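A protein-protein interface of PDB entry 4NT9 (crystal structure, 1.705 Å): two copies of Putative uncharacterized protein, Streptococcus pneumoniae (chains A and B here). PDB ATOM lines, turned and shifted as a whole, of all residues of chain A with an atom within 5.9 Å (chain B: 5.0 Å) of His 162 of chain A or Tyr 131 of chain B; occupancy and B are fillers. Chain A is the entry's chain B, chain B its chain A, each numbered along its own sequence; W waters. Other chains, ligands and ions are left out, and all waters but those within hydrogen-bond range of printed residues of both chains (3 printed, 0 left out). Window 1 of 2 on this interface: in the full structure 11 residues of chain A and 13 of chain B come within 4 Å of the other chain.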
ATOM      1  N   LEU A  82       8.172  -9.164 -38.312  1.00  0.00           N
ATOM      2  CA  LEU A  82       9.166  -9.839 -37.480  1.00  0.00           C
ATOM      3  C   LEU A  82      10.151  -8.814 -36.937  1.00  0.00           C
ATOM      4  O   LEU A  82      10.543  -8.883 -35.750  1.00  0.00           O
ATOM      5  CB  LEU A  82       9.890 -10.949 -38.304  1.00  0.00           C
ATOM      6  CG  LEU A  82      11.061 -11.698 -37.634  1.00  0.00           C
ATOM      7  CD1 LEU A  82      11.252 -13.108 -38.225  1.00  0.00           C
ATOM      8  CD2 LEU A  82      12.386 -10.914 -37.739  1.00  0.00           C
ATOM      9  N   ALA A  85       8.442  -6.983 -34.106  1.00  0.00           N
ATOM     10  CA  ALA A  85       8.498  -7.860 -32.937  1.00  0.00           C
ATOM     11  C   ALA A  85       9.877  -7.898 -32.253  1.00  0.00           C
ATOM     12  O   ALA A  85       9.950  -7.833 -31.005  1.00  0.00           O
ATOM     13  CB  ALA A  85       8.044  -9.244 -33.320  1.00  0.00           C
ATOM     14  N   ALA A  89      10.967  -6.534 -28.517  1.00  0.00           N
ATOM     15  CA  ALA A  89      11.571  -7.438 -27.545  1.00  0.00           C
ATOM     16  C   ALA A  89      12.857  -6.846 -26.985  1.00  0.00           C
ATOM     17  O   ALA A  89      13.551  -7.490 -26.188  1.00  0.00           O
ATOM     18  CB  ALA A  89      11.827  -8.799 -28.148  1.00  0.00           C
ATOM     19  N   GLN A 157      19.375 -16.166 -31.093  1.00  0.00           N
ATOM     20  CA  GLN A 157      18.429 -17.124 -30.514  1.00  0.00           C
ATOM     21  C   GLN A 157      16.951 -16.711 -30.641  1.00  0.00           C
ATOM     22  O   GLN A 157      16.076 -17.567 -30.824  1.00  0.00           O
ATOM     23  CB  GLN A 157      18.797 -17.399 -29.043  1.00  0.00           C
ATOM     24  CG  GLN A 157      18.041 -18.591 -28.446  1.00  0.00           C
ATOM     25  CD  GLN A 157      18.387 -19.903 -29.146  1.00  0.00           C
ATOM     26  OE1 GLN A 157      19.562 -20.266 -29.280  1.00  0.00           O
ATOM     27  NE2 GLN A 157      17.383 -20.613 -29.599  1.00  0.00           N
ATOM     28  N   TRP A 158      16.667 -15.415 -30.570  1.00  0.00           N
ATOM     29  CA  TRP A 158      15.288 -14.956 -30.775  1.00  0.00           C
ATOM     30  C   TRP A 158      14.822 -15.367 -32.188  1.00  0.00           C
ATOM     31  O   TRP A 158      13.728 -15.893 -32.351  1.00  0.00           O
ATOM     32  CB  TRP A 158      15.201 -13.425 -30.612  1.00  0.00           C
ATOM     33  CG  TRP A 158      13.762 -12.888 -30.650  1.00  0.00           C
ATOM     34  CD1 TRP A 158      12.978 -12.572 -29.567  1.00  0.00           C
ATOM     35  CD2 TRP A 158      12.947 -12.608 -31.823  1.00  0.00           C
ATOM     36  NE1 TRP A 158      11.745 -12.141 -29.974  1.00  0.00           N
ATOM     37  CE2 TRP A 158      11.691 -12.144 -31.346  1.00  0.00           C
ATOM     38  CE3 TRP A 158      13.147 -12.734 -33.208  1.00  0.00           C
ATOM     39  CZ2 TRP A 158      10.640 -11.791 -32.193  1.00  0.00           C
ATOM     40  CZ3 TRP A 158      12.085 -12.387 -34.070  1.00  0.00           C
ATOM     41  CH2 TRP A 158      10.846 -11.914 -33.548  1.00  0.00           C
ATOM     42  N   LEU A 159      15.672 -15.123 -33.185  1.00  0.00           N
ATOM     43  CA  LEU A 159      15.362 -15.557 -34.568  1.00  0.00           C
ATOM     44  C   LEU A 159      15.121 -17.053 -34.594  1.00  0.00           C
ATOM     45  O   LEU A 159      14.125 -17.530 -35.141  1.00  0.00           O
ATOM     46  CB  LEU A 159      16.502 -15.177 -35.534  1.00  0.00           C
ATOM     47  CG  LEU A 159      16.501 -13.669 -35.734  1.00  0.00           C
ATOM     48  CD1 LEU A 159      17.816 -13.280 -36.383  1.00  0.00           C
ATOM     49  CD2 LEU A 159      15.314 -13.241 -36.611  1.00  0.00           C
ATOM     50  N   LEU A 160      15.985 -17.834 -33.961  1.00  0.00           N
ATOM     51  CA  LEU A 160      15.704 -19.274 -33.962  1.00  0.00           C
ATOM     52  C   LEU A 160      14.363 -19.625 -33.282  1.00  0.00           C
ATOM     53  O   LEU A 160      13.626 -20.522 -33.738  1.00  0.00           O
ATOM     54  CB  LEU A 160      16.848 -20.049 -33.299  1.00  0.00           C
ATOM     55  CG  LEU A 160      18.210 -20.052 -34.014  1.00  0.00           C
ATOM     56  CD1 LEU A 160      19.244 -20.598 -32.990  1.00  0.00           C
ATOM     57  CD2 LEU A 160      18.240 -20.874 -35.283  1.00  0.00           C
ATOM     58  N   ASP A 161      14.013 -18.924 -32.213  1.00  0.00           N
ATOM     59  CA  ASP A 161      12.830 -19.310 -31.448  1.00  0.00           C
ATOM     60  C   ASP A 161      11.524 -18.794 -32.057  1.00  0.00           C
ATOM     61  O   ASP A 161      10.464 -19.420 -31.856  1.00  0.00           O
ATOM     62  CB  ASP A 161      12.927 -18.735 -30.028  1.00  0.00           C
ATOM     63  CG  ASP A 161      14.026 -19.390 -29.184  1.00  0.00           C
ATOM     64  OD1 ASP A 161      14.428 -20.531 -29.486  1.00  0.00           O
ATOM     65  OD2 ASP A 161      14.448 -18.752 -28.181  1.00  0.00           O
ATOM     66  N   HIS A 162      11.588 -17.665 -32.772  1.00  0.00           N
ATOM     67  CA  HIS A 162      10.392 -16.957 -33.201  1.00  0.00           C
ATOM     68  C   HIS A 162      10.200 -16.880 -34.707  1.00  0.00           C
ATOM     69  O   HIS A 162       9.099 -16.608 -35.137  1.00  0.00           O
ATOM     70  CB  HIS A 162      10.429 -15.498 -32.716  1.00  0.00           C
ATOM     71  CG  HIS A 162      10.277 -15.340 -31.240  1.00  0.00           C
ATOM     72  ND1 HIS A 162       9.062 -15.028 -30.664  1.00  0.00           N
ATOM     73  CD2 HIS A 162      11.161 -15.436 -30.224  1.00  0.00           C
ATOM     74  CE1 HIS A 162       9.208 -14.925 -29.360  1.00  0.00           C
ATOM     75  NE2 HIS A 162      10.476 -15.174 -29.059  1.00  0.00           N
ATOM     76  N   ALA A 163      11.267 -17.039 -35.492  1.00  0.00           N
ATOM     77  CA  ALA A 163      11.123 -16.766 -36.954  1.00  0.00           C
ATOM     78  C   ALA A 163      10.003 -17.514 -37.668  1.00  0.00           C
ATOM     79  O   ALA A 163       9.367 -16.963 -38.571  1.00  0.00           O
ATOM     80  CB  ALA A 163      12.457 -16.973 -37.683  1.00  0.00           C
ATOM     81  N   ALA A 164       9.753 -18.754 -37.263  1.00  0.00           N
ATOM     82  CA  ALA A 164       8.765 -19.616 -37.929  1.00  0.00           C
ATOM     83  C   ALA A 164       7.359 -19.067 -37.749  1.00  0.00           C
ATOM     84  O   ALA A 164       6.458 -19.378 -38.539  1.00  0.00           O
ATOM     85  CB  ALA A 164       8.857 -21.035 -37.384  1.00  0.00           C
ATOM     86  N   ASP A 165       7.155 -18.282 -36.692  1.00  0.00           N
ATOM     87  CA  ASP A 165       5.847 -17.662 -36.465  1.00  0.00           C
ATOM     88  C   ASP A 165       5.511 -16.691 -37.603  1.00  0.00           C
ATOM     89  O   ASP A 165       4.331 -16.365 -37.798  1.00  0.00           O
ATOM     90  CB  ASP A 165       5.806 -16.874 -35.139  1.00  0.00           C
ATOM     91  CG  ASP A 165       5.898 -17.756 -33.904  1.00  0.00           C
ATOM     92  OD1 ASP A 165       5.809 -18.999 -33.989  1.00  0.00           O
ATOM     93  OD2 ASP A 165       6.034 -17.170 -32.818  1.00  0.00           O
ATOM     94  N   TYR A 166       6.539 -16.224 -38.317  1.00  0.00           N
ATOM     95  CA  TYR A 166       6.385 -15.299 -39.458  1.00  0.00           C
ATOM     96  C   TYR A 166       6.672 -15.971 -40.806  1.00  0.00           C
ATOM     97  O   TYR A 166       6.769 -15.297 -41.826  1.00  0.00           O
ATOM     98  CB  TYR A 166       7.291 -14.062 -39.260  1.00  0.00           C
ATOM     99  CG  TYR A 166       6.997 -13.377 -37.954  1.00  0.00           C
ATOM    100  CD1 TYR A 166       7.613 -13.783 -36.754  1.00  0.00           C
ATOM    101  CD2 TYR A 166       6.034 -12.386 -37.901  1.00  0.00           C
ATOM    102  CE1 TYR A 166       7.283 -13.167 -35.556  1.00  0.00           C
ATOM    103  CE2 TYR A 166       5.691 -11.777 -36.693  1.00  0.00           C
ATOM    104  CZ  TYR A 166       6.319 -12.177 -35.546  1.00  0.00           C
ATOM    105  OH  TYR A 166       5.964 -11.542 -34.375  1.00  0.00           O
ATOM    106  N   ASN B  58       3.569 -10.315 -21.257  1.00  0.00           N
ATOM    107  CA  ASN B  58       2.903 -11.475 -21.861  1.00  0.00           C
ATOM    108  C   ASN B  58       3.436 -11.638 -23.264  1.00  0.00           C
ATOM    109  O   ASN B  58       4.475 -11.069 -23.584  1.00  0.00           O
ATOM    110  CB  ASN B  58       1.355 -11.380 -21.785  1.00  0.00           C
ATOM    111  CG  ASN B  58       0.744 -10.239 -22.656  1.00  0.00           C
ATOM    112  OD1 ASN B  58       1.378  -9.711 -23.578  1.00  0.00           O
ATOM    113  ND2 ASN B  58      -0.514  -9.910 -22.386  1.00  0.00           N
ATOM    114  N   LYS B  59       2.760 -12.406 -24.104  1.00  0.00           N
ATOM    115  CA  LYS B  59       3.351 -12.751 -25.387  1.00  0.00           C
ATOM    116  C   LYS B  59       3.275 -11.583 -26.361  1.00  0.00           C
ATOM    117  O   LYS B  59       3.940 -11.595 -27.383  1.00  0.00           O
ATOM    118  CB  LYS B  59       2.692 -14.002 -25.943  1.00  0.00           C
ATOM    119  CG  LYS B  59       2.992 -15.226 -25.070  1.00  0.00           C
ATOM    120  CD  LYS B  59       2.339 -16.495 -25.589  1.00  0.00           C
ATOM    121  CE  LYS B  59       2.720 -17.671 -24.696  1.00  0.00           C
ATOM    122  NZ  LYS B  59       2.097 -18.930 -25.164  1.00  0.00           N
ATOM    123  N   PRO B  62       6.632  -8.178 -24.238  1.00  0.00           N
ATOM    124  CA  PRO B  62       7.765  -8.907 -23.643  1.00  0.00           C
ATOM    125  C   PRO B  62       8.558  -8.037 -22.665  1.00  0.00           C
ATOM    126  O   PRO B  62       8.399  -6.827 -22.667  1.00  0.00           O
ATOM    127  CB  PRO B  62       8.679  -9.215 -24.865  1.00  0.00           C
ATOM    128  CG  PRO B  62       8.305  -8.129 -25.879  1.00  0.00           C
ATOM    129  CD  PRO B  62       6.828  -7.897 -25.674  1.00  0.00           C
ATOM    130  N   LEU B  63       9.427  -8.665 -21.885  1.00  0.00           N
ATOM    131  CA  LEU B  63      10.446  -7.955 -21.134  1.00  0.00           C
ATOM    132  C   LEU B  63      11.741  -7.951 -21.915  1.00  0.00           C
ATOM    133  O   LEU B  63      12.070  -8.927 -22.564  1.00  0.00           O
ATOM    134  CB  LEU B  63      10.662  -8.637 -19.791  1.00  0.00           C
ATOM    135  CG  LEU B  63       9.332  -8.685 -19.039  1.00  0.00           C
ATOM    136  CD1 LEU B  63       9.366  -9.682 -17.908  1.00  0.00           C
ATOM    137  CD2 LEU B  63       8.995  -7.317 -18.478  1.00  0.00           C
ATOM    138  N   LYS B 119       9.989 -28.701 -29.708  1.00  0.00           N
ATOM    139  CA  LYS B 119       9.557 -27.311 -29.758  1.00  0.00           C
ATOM    140  C   LYS B 119       8.063 -27.101 -29.548  1.00  0.00           C
ATOM    141  O   LYS B 119       7.663 -26.138 -28.891  1.00  0.00           O
ATOM    142  CB  LYS B 119       9.958 -26.687 -31.100  1.00  0.00           C
ATOM    143  CG  LYS B 119       9.436 -25.253 -31.262  1.00  0.00           C
ATOM    144  CD  LYS B 119      10.579 -24.271 -31.422  1.00  0.00           C
ATOM    145  CE  LYS B 119      10.059 -22.828 -31.483  1.00  0.00           C
ATOM    146  NZ  LYS B 119      10.847 -22.016 -30.576  1.00  0.00           N
ATOM    147  N   ALA B 127       7.530 -20.792 -21.835  1.00  0.00           N
ATOM    148  CA  ALA B 127       7.436 -19.503 -22.495  1.00  0.00           C
ATOM    149  C   ALA B 127       8.829 -19.192 -23.038  1.00  0.00           C
ATOM    150  O   ALA B 127       9.841 -19.505 -22.404  1.00  0.00           O
ATOM    151  CB  ALA B 127       7.007 -18.433 -21.519  1.00  0.00           C
ATOM    152  N   ARG B 128       8.898 -18.555 -24.204  1.00  0.00           N
ATOM    153  CA  ARG B 128      10.189 -18.111 -24.733  1.00  0.00           C
ATOM    154  C   ARG B 128      10.781 -17.013 -23.843  1.00  0.00           C
ATOM    155  O   ARG B 128      10.050 -16.265 -23.204  1.00  0.00           O
ATOM    156  CB  ARG B 128       9.979 -17.614 -26.163  1.00  0.00           C
ATOM    157  CG  ARG B 128       9.524 -18.719 -27.091  1.00  0.00           C
ATOM    158  CD  ARG B 128       8.996 -18.150 -28.417  1.00  0.00           C
ATOM    159  NE  ARG B 128       8.295 -19.186 -29.181  1.00  0.00           N
ATOM    160  CZ  ARG B 128       7.609 -18.959 -30.304  1.00  0.00           C
ATOM    161  NH1 ARG B 128       7.530 -17.736 -30.818  1.00  0.00           N
ATOM    162  NH2 ARG B 128       6.972 -19.952 -30.896  1.00  0.00           N
ATOM    163  N   PRO B 129      12.120 -16.911 -23.775  1.00  0.00           N
ATOM    164  CA  PRO B 129      12.695 -15.906 -22.860  1.00  0.00           C
ATOM    165  C   PRO B 129      12.290 -14.485 -23.224  1.00  0.00           C
ATOM    166  O   PRO B 129      12.251 -14.152 -24.423  1.00  0.00           O
ATOM    167  CB  PRO B 129      14.219 -16.070 -23.052  1.00  0.00           C
ATOM    168  CG  PRO B 129      14.371 -16.836 -24.330  1.00  0.00           C
ATOM    169  CD  PRO B 129      13.161 -17.717 -24.440  1.00  0.00           C
ATOM    170  N   GLY B 130      11.968 -13.690 -22.202  1.00  0.00           N
ATOM    171  CA  GLY B 130      11.432 -12.337 -22.330  1.00  0.00           C
ATOM    172  C   GLY B 130       9.905 -12.333 -22.340  1.00  0.00           C
ATOM    173  O   GLY B 130       9.267 -11.274 -22.271  1.00  0.00           O
ATOM    174  N   TYR B 131       9.311 -13.522 -22.444  1.00  0.00           N
ATOM    175  CA  TYR B 131       7.857 -13.647 -22.538  1.00  0.00           C
ATOM    176  C   TYR B 131       7.285 -14.453 -21.370  1.00  0.00           C
ATOM    177  O   TYR B 131       6.186 -15.002 -21.463  1.00  0.00           O
ATOM    178  CB  TYR B 131       7.466 -14.317 -23.858  1.00  0.00           C
ATOM    179  CG  TYR B 131       7.948 -13.544 -25.077  1.00  0.00           C
ATOM    180  CD1 TYR B 131       9.264 -13.667 -25.532  1.00  0.00           C
ATOM    181  CD2 TYR B 131       7.103 -12.658 -25.737  1.00  0.00           C
ATOM    182  CE1 TYR B 131       9.721 -12.925 -26.679  1.00  0.00           C
ATOM    183  CE2 TYR B 131       7.517 -11.953 -26.863  1.00  0.00           C
ATOM    184  CZ  TYR B 131       8.841 -12.086 -27.320  1.00  0.00           C
ATOM    185  OH  TYR B 131       9.300 -11.385 -28.412  1.00  0.00           O
ATOM    186  N   SER B 132       8.029 -14.543 -20.270  1.00  0.00           N
ATOM    187  CA  SER B 132       7.492 -15.176 -19.057  1.00  0.00           C
ATOM    188  C   SER B 132       7.272 -14.133 -17.969  1.00  0.00           C
ATOM    189  O   SER B 132       8.115 -13.290 -17.762  1.00  0.00           O
ATOM    190  CB  SER B 132       8.423 -16.273 -18.523  1.00  0.00           C
ATOM    191  OG  SER B 132       8.027 -16.661 -17.188  1.00  0.00           O
ATOM    192  N   GLU B 133       6.145 -14.199 -17.258  1.00  0.00           N
ATOM    193  CA  GLU B 133       5.930 -13.244 -16.176  1.00  0.00           C
ATOM    194  C   GLU B 133       6.945 -13.408 -15.046  1.00  0.00           C
ATOM    195  O   GLU B 133       7.125 -12.514 -14.241  1.00  0.00           O
ATOM    196  CB  GLU B 133       4.504 -13.423 -15.617  1.00  0.00           C
ATOM    197  CG  GLU B 133       3.972 -12.163 -14.950  1.00  0.00           C
ATOM    198  CD  GLU B 133       2.527 -12.291 -14.512  1.00  0.00           C
ATOM    199  OE1 GLU B 133       1.781 -11.283 -14.707  1.00  0.00           O
ATOM    200  OE2 GLU B 133       2.144 -13.359 -13.922  1.00  0.00           O
ATOM    201  N   GLN B 135       9.979 -13.257 -15.117  1.00  0.00           N
ATOM    202  CA  GLN B 135      11.092 -12.304 -15.255  1.00  0.00           C
ATOM    203  C   GLN B 135      10.769 -10.966 -14.586  1.00  0.00           C
ATOM    204  O   GLN B 135      11.660 -10.138 -14.385  1.00  0.00           O
ATOM    205  CB  GLN B 135      11.493 -12.143 -16.747  1.00  0.00           C
ATOM    206  CG  GLN B 135      12.772 -11.329 -16.968  1.00  0.00           C
ATOM    207  CD  GLN B 135      13.080 -11.132 -18.442  1.00  0.00           C
ATOM    208  OE1 GLN B 135      12.580 -11.886 -19.291  1.00  0.00           O
ATOM    209  NE2 GLN B 135      13.899 -10.117 -18.765  1.00  0.00           N
ATOM    210  N   TYR B 182      -1.573 -18.254 -22.327  1.00  0.00           N
ATOM    211  CA  TYR B 182      -0.827 -19.283 -21.599  1.00  0.00           C
ATOM    212  C   TYR B 182      -1.732 -20.384 -21.116  1.00  0.00           C
ATOM    213  O   TYR B 182      -2.904 -20.177 -20.741  1.00  0.00           O
ATOM    214  CB  TYR B 182      -0.110 -18.688 -20.359  1.00  0.00           C
ATOM    215  CG  TYR B 182       0.871 -17.586 -20.681  1.00  0.00           C
ATOM    216  CD1 TYR B 182       0.438 -16.328 -21.019  1.00  0.00           C
ATOM    217  CD2 TYR B 182       2.247 -17.818 -20.627  1.00  0.00           C
ATOM    218  CE1 TYR B 182       1.327 -15.310 -21.319  1.00  0.00           C
ATOM    219  CE2 TYR B 182       3.158 -16.809 -20.902  1.00  0.00           C
ATOM    220  CZ  TYR B 182       2.686 -15.559 -21.263  1.00  0.00           C
ATOM    221  OH  TYR B 182       3.588 -14.556 -21.548  1.00  0.00           O
ATOM    222  N   TYR B 217       1.703 -15.736 -29.463  1.00  0.00           N
ATOM    223  CA  TYR B 217       2.666 -14.831 -30.071  1.00  0.00           C
ATOM    224  C   TYR B 217       2.074 -14.392 -31.422  1.00  0.00           C
ATOM    225  O   TYR B 217       1.276 -15.111 -32.013  1.00  0.00           O
ATOM    226  CB  TYR B 217       4.028 -15.504 -30.319  1.00  0.00           C
ATOM    227  CG  TYR B 217       4.655 -16.172 -29.120  1.00  0.00           C
ATOM    228  CD1 TYR B 217       5.372 -15.424 -28.181  1.00  0.00           C
ATOM    229  CD2 TYR B 217       4.552 -17.541 -28.919  1.00  0.00           C
ATOM    230  CE1 TYR B 217       5.974 -16.025 -27.084  1.00  0.00           C
ATOM    231  CE2 TYR B 217       5.144 -18.157 -27.785  1.00  0.00           C
ATOM    232  CZ  TYR B 217       5.854 -17.368 -26.880  1.00  0.00           C
ATOM    233  OH  TYR B 217       6.454 -17.920 -25.768  1.00  0.00           O
HETATM  234  O   HOH W   1       8.071  -9.403 -29.436  1.00  0.00           O
HETATM  235  O   HOH W   2      12.883  -9.786 -24.880  1.00  0.00           O
HETATM  236  O   HOH W   3      12.444 -15.161 -26.963  1.00  0.00           O
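NH1 of Arg 128 of chain B lies within salt-bridge range of OD2 of Asp 165 of chain A (2.6 Å).
NE of Arg 128 of chain B sits close to O of Asp 161 of chain A (3.5 Å).
The side-chain hydroxyl (OH) of Tyr 131 of chain B is in hydrogen-bond range of the indole nitrogen (NE1) of Trp 158 of chain A (3.0 Å).
A ring nitrogen (ND1) of His 162 of chain A lies within hydrogen-bond range of the guanidinium group of Arg 128 of chain B (3.1 Å).
O of Asp 161 of chain A sits at hydrogen-bond distance from NZ of Lys 119 of chain B (2.9 Å).
O of Tyr 131 of chain B lies within hydrogen-bond range of OH of Tyr 182 of chain B (2.6 Å).
The indole nitrogen (NE1) of Trp 158 of chain A sits close to a ring nitrogen (NE2) of His 162 of chain A (3.4 Å).
The side-chain hydroxyl (OH) of Tyr 217 of chain B lies within hydrogen-bond range of the backbone NH (N) of Arg 128 of chain B (3.0 Å).
NE2 of Gln 157 of chain A is in hydrogen-bond range of OD1 of Asp 161 of chain A, at 3.0 Å.
Ala 89 of chain A touches Pro 62 of chain B.
OH of Tyr 131 of chain B touches CB of Ala 89 of chain A (3.6 Å).
His 162 of chain A touches Tyr 131 of chain B.
Asp 165 of chain A touches Tyr 217 of chain B (OD2 to CB, 3.6 Å).
Of the printed residues of chain B, Ala 89 of chain A touches Pro 62 and Tyr 131.
Gln 157 of chain A touches none of the printed residues of chain B.
Printed residues of chain B within 4 Å of Asp 161 of chain A: Lys 119 and Arg 128.
His 162 of chain A touches two residues of chain B.
Printed residues of chain A within 4 Å of Pro 62 of chain B: Ala 89 (3.7 Å).
Tyr 131 of chain B touches just these residues of chain A: Ala 89, Trp 158 and His 162.
The nearest residue of chain A that does not touch Tyr 131 of chain B is Ala 85 of chain A (4.4 Å).
The nearest printed residue of chain A that does not touch Pro 62 of chain B is Ala 85 of chain A (5.4 Å).
Printed residues of chain A that touch a printed residue of chain B: Ala 89, Trp 158, Asp 161, His 162 and Asp 165.
Hydrophobic or aromatic side chains of chain B within 4 Å of the printed part of chain A: Pro 62, Tyr 131 and Tyr 217.
Among the printed residues, Asp or Glu carboxylates within 4 Å of a Lys or Arg side-chain nitrogen of the other chain: Asp 165 of chain A with Arg 128 of chain B.
No position is printed for both chains.
Of the 9 pairs that touch across the chains among the printed residues, none has its exchanged pair printed and touching as well.
Water W1 bridges OH of Tyr 131 of chain B (2.5 Å) and O of Ala 85 of chain A (2.9 Å).
Water W2 bridges the backbone carbonyl oxygen of Leu 63 of chain B (2.6 Å) and the backbone carbonyl oxygen of Ala 89 of chain A (2.7 Å).
Water W3 bridges the backbone carbonyl oxygen of Pro 129 of chain B (2.7 Å) and a ring nitrogen (NE2) of His 162 of chain A (2.9 Å).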
